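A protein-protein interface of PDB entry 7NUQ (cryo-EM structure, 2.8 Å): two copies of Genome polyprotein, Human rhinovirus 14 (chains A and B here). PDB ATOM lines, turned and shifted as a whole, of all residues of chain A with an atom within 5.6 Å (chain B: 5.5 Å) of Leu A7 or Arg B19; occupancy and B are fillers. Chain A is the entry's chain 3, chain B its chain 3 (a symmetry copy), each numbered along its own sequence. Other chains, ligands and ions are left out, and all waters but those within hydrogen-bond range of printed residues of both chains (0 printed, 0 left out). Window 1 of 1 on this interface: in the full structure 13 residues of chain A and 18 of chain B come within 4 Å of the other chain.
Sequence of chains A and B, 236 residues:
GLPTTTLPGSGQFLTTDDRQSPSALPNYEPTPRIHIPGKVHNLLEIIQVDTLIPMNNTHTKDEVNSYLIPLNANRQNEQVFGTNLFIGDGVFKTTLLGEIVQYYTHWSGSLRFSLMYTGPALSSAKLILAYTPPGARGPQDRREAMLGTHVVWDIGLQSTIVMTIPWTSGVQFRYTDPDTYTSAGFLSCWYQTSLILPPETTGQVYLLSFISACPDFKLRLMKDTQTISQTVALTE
The side-chain hydroxyl (OG1) of Thr A6 lies close to the backbone NH (N) of Gly B11, 2.3 Å away.
OG of Ser A10 lies within hydrogen-bond range of O of Leu A7, 2.5 Å away.
Among the printed residues, pairs that only touch across the chains: Pro A8 with Gln B12 (3.1 Å), Leu A7 with Arg B19 (3.8 Å), Leu A7 with Asp B17 (3.9 Å) and Thr A6 with Gln B12 (3.999 Å).
Of chain B, only Asp B17 and Arg B19 come within 4 Å of Leu A7.
Of chain A, only Leu A7 comes within 4 Å of Arg B19.
Of the printed residues of chain A, Asp B17 touches Leu A7 (3.9 Å).
Printed residues of chain B within 4 Å of Thr A6: Gly B11 (2.3 Å) and Gln B12 (3.999 Å).
Of the printed residues of chain A, Gly B11 touches Thr A6.
Of the printed residues of chain B, Pro A8 touches Gln B12 (3.1 Å).
Asp B18 touches none of the printed residues of chain A.
Gln B20 touches none of the printed residues of chain A.
The nearest residue of chain B that does not touch Leu A7 is Gly B11 (4.2 Å).
The nearest printed residue of chain A that does not touch Arg B19 is Pro A8 (6.3 Å).
The nearest printed residue of chain B that does not touch Thr A6 is Asp B17 (7.4 Å).
Of the 7 printed residues of chain B, 4 touch a printed residue of chain A.
Hydrophobic or aromatic side chains of chain A that line the printed part of chain B: Leu A7 and Pro A8.
Among the printed residues, 5 pairs touch across the chains.
Among the printed residues, no Asp or Glu carboxylate lies within 4 Å of a Lys or Arg side-chain nitrogen of the other chain.
No position is printed for both chains.
Of the 5 pairs that touch across the chains among the printed residues, none has its exchanged pair printed and touching as well.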
ATOM      1  N   THR A   5      17.119 -21.829 -16.055  1.00  0.00           N
ATOM      2  CA  THR A   5      17.145 -22.816 -14.982  1.00  0.00           C
ATOM      3  C   THR A   5      18.529 -22.803 -14.355  1.00  0.00           C
ATOM      4  O   THR A   5      19.519 -23.114 -15.027  1.00  0.00           O
ATOM      5  CB  THR A   5      16.802 -24.216 -15.503  1.00  0.00           C
ATOM      6  OG1 THR A   5      15.515 -24.194 -16.132  1.00  0.00           O
ATOM      7  CG2 THR A   5      16.791 -25.225 -14.365  1.00  0.00           C
ATOM      8  N   THR A   6      18.599 -22.446 -13.076  1.00  0.00           N
ATOM      9  CA  THR A   6      19.874 -22.354 -12.376  1.00  0.00           C
ATOM     10  C   THR A   6      20.418 -23.755 -12.119  1.00  0.00           C
ATOM     11  O   THR A   6      19.807 -24.542 -11.388  1.00  0.00           O
ATOM     12  CB  THR A   6      19.709 -21.594 -11.061  1.00  0.00           C
ATOM     13  OG1 THR A   6      18.734 -22.252 -10.242  1.00  0.00           O
ATOM     14  CG2 THR A   6      19.267 -20.160 -11.324  1.00  0.00           C
ATOM     15  N   LEU A   7      21.564 -24.062 -12.720  1.00  0.00           N
ATOM     16  CA  LEU A   7      22.197 -25.352 -12.513  1.00  0.00           C
ATOM     17  C   LEU A   7      22.798 -25.423 -11.111  1.00  0.00           C
ATOM     18  O   LEU A   7      23.062 -24.392 -10.485  1.00  0.00           O
ATOM     19  CB  LEU A   7      23.280 -25.581 -13.564  1.00  0.00           C
ATOM     20  CG  LEU A   7      22.805 -25.626 -15.018  1.00  0.00           C
ATOM     21  CD1 LEU A   7      23.987 -25.779 -15.962  1.00  0.00           C
ATOM     22  CD2 LEU A   7      21.801 -26.752 -15.228  1.00  0.00           C
ATOM     23  N   PRO A   8      23.019 -26.628 -10.589  1.00  0.00           N
ATOM     24  CA  PRO A   8      23.627 -26.745  -9.260  1.00  0.00           C
ATOM     25  C   PRO A   8      24.997 -26.085  -9.215  1.00  0.00           C
ATOM     26  O   PRO A   8      25.782 -26.157 -10.164  1.00  0.00           O
ATOM     27  CB  PRO A   8      23.730 -28.262  -9.042  1.00  0.00           C
ATOM     28  CG  PRO A   8      23.610 -28.864 -10.403  1.00  0.00           C
ATOM     29  CD  PRO A   8      22.718 -27.947 -11.172  1.00  0.00           C
ATOM     30  N   GLY A   9      25.273 -25.434  -8.090  1.00  0.00           N
ATOM     31  CA  GLY A   9      26.509 -24.696  -7.927  1.00  0.00           C
ATOM     32  C   GLY A   9      26.461 -23.267  -8.414  1.00  0.00           C
ATOM     33  O   GLY A   9      27.512 -22.706  -8.745  1.00  0.00           O
ATOM     34  N   SER A  10      25.279 -22.658  -8.472  1.00  0.00           N
ATOM     35  CA  SER A  10      25.134 -21.283  -8.931  1.00  0.00           C
ATOM     36  C   SER A  10      25.445 -20.325  -7.789  1.00  0.00           C
ATOM     37  O   SER A  10      25.003 -20.536  -6.655  1.00  0.00           O
ATOM     38  CB  SER A  10      23.719 -21.039  -9.459  1.00  0.00           C
ATOM     39  OG  SER A  10      23.430 -21.890 -10.553  1.00  0.00           O
ATOM     40  N   GLY B  11      18.469 -24.387  -9.448  1.00  0.00           N
ATOM     41  CA  GLY B  11      19.428 -24.618  -8.390  1.00  0.00           C
ATOM     42  C   GLY B  11      19.422 -26.014  -7.811  1.00  0.00           C
ATOM     43  O   GLY B  11      20.113 -26.255  -6.815  1.00  0.00           O
ATOM     44  N   GLN B  12      18.666 -26.938  -8.397  1.00  0.00           N
ATOM     45  CA  GLN B  12      18.600 -28.301  -7.889  1.00  0.00           C
ATOM     46  C   GLN B  12      19.773 -29.118  -8.411  1.00  0.00           C
ATOM     47  O   GLN B  12      20.303 -28.855  -9.495  1.00  0.00           O
ATOM     48  CB  GLN B  12      17.283 -28.959  -8.300  1.00  0.00           C
ATOM     49  CG  GLN B  12      17.148 -29.197  -9.797  1.00  0.00           C
ATOM     50  CD  GLN B  12      15.779 -29.719 -10.184  1.00  0.00           C
ATOM     51  OE1 GLN B  12      14.888 -29.845  -9.343  1.00  0.00           O
ATOM     52  NE2 GLN B  12      15.603 -30.028 -11.463  1.00  0.00           N
ATOM     53  N   ASP B  17      21.883 -35.265 -14.472  1.00  0.00           N
ATOM     54  CA  ASP B  17      22.019 -34.170 -15.423  1.00  0.00           C
ATOM     55  C   ASP B  17      23.466 -34.042 -15.883  1.00  0.00           C
ATOM     56  O   ASP B  17      24.391 -34.020 -15.065  1.00  0.00           O
ATOM     57  CB  ASP B  17      21.543 -32.862 -14.791  1.00  0.00           C
ATOM     58  CG  ASP B  17      21.393 -31.745 -15.806  1.00  0.00           C
ATOM     59  OD1 ASP B  17      21.615 -31.998 -17.008  1.00  0.00           O
ATOM     60  OD2 ASP B  17      21.053 -30.614 -15.399  1.00  0.00           O
ATOM     61  N   ASP B  18      23.660 -33.958 -17.201  1.00  0.00           N
ATOM     62  CA  ASP B  18      24.991 -33.848 -17.798  1.00  0.00           C
ATOM     63  C   ASP B  18      25.100 -32.479 -18.465  1.00  0.00           C
ATOM     64  O   ASP B  18      24.691 -32.275 -19.607  1.00  0.00           O
ATOM     65  CB  ASP B  18      25.225 -34.988 -18.785  1.00  0.00           C
ATOM     66  CG  ASP B  18      26.650 -35.026 -19.310  1.00  0.00           C
ATOM     67  OD1 ASP B  18      27.281 -33.954 -19.422  1.00  0.00           O
ATOM     68  OD2 ASP B  18      27.140 -36.135 -19.609  1.00  0.00           O
ATOM     69  N   ARG B  19      25.676 -31.532 -17.729  1.00  0.00           N
ATOM     70  CA  ARG B  19      25.849 -30.165 -18.196  1.00  0.00           C
ATOM     71  C   ARG B  19      27.320 -29.772 -18.171  1.00  0.00           C
ATOM     72  O   ARG B  19      28.186 -30.528 -17.719  1.00  0.00           O
ATOM     73  CB  ARG B  19      25.042 -29.186 -17.337  1.00  0.00           C
ATOM     74  CG  ARG B  19      23.564 -29.533 -17.206  1.00  0.00           C
ATOM     75  CD  ARG B  19      22.885 -29.660 -18.564  1.00  0.00           C
ATOM     76  NE  ARG B  19      23.091 -28.482 -19.400  1.00  0.00           N
ATOM     77  CZ  ARG B  19      22.678 -28.374 -20.660  1.00  0.00           C
ATOM     78  NH1 ARG B  19      22.031 -29.377 -21.240  1.00  0.00           N
ATOM     79  NH2 ARG B  19      22.912 -27.262 -21.341  1.00  0.00           N
ATOM     80  N   GLN B  20      27.590 -28.565 -18.667  1.00  0.00           N
ATOM     81  CA  GLN B  20      28.944 -28.027 -18.680  1.00  0.00           C
ATOM     82  C   GLN B  20      29.371 -27.633 -17.269  1.00  0.00           C
ATOM     83  O   GLN B  20      28.555 -27.575 -16.345  1.00  0.00           O
ATOM     84  CB  GLN B  20      29.025 -26.811 -19.602  1.00  0.00           C
ATOM     85  CG  GLN B  20      28.379 -26.997 -20.969  1.00  0.00           C
ATOM     86  CD  GLN B  20      28.403 -25.727 -21.802  1.00  0.00           C
ATOM     87  OE1 GLN B  20      29.405 -25.010 -21.834  1.00  0.00           O
ATOM     88  NE2 GLN B  20      27.293 -25.439 -22.475  1.00  0.00           N
ATOM     89  N   SER B  21      30.663 -27.360 -17.104  1.00  0.00           N
ATOM     90  CA  SER B  21      31.196 -26.992 -15.799  1.00  0.00           C
ATOM     91  C   SER B  21      32.491 -26.213 -15.976  1.00  0.00           C
ATOM     92  O   SER B  21      33.348 -26.619 -16.769  1.00  0.00           O
ATOM     93  CB  SER B  21      31.451 -28.232 -14.932  1.00  0.00           C
ATOM     94  OG  SER B  21      30.302 -29.056 -14.870  1.00  0.00           O
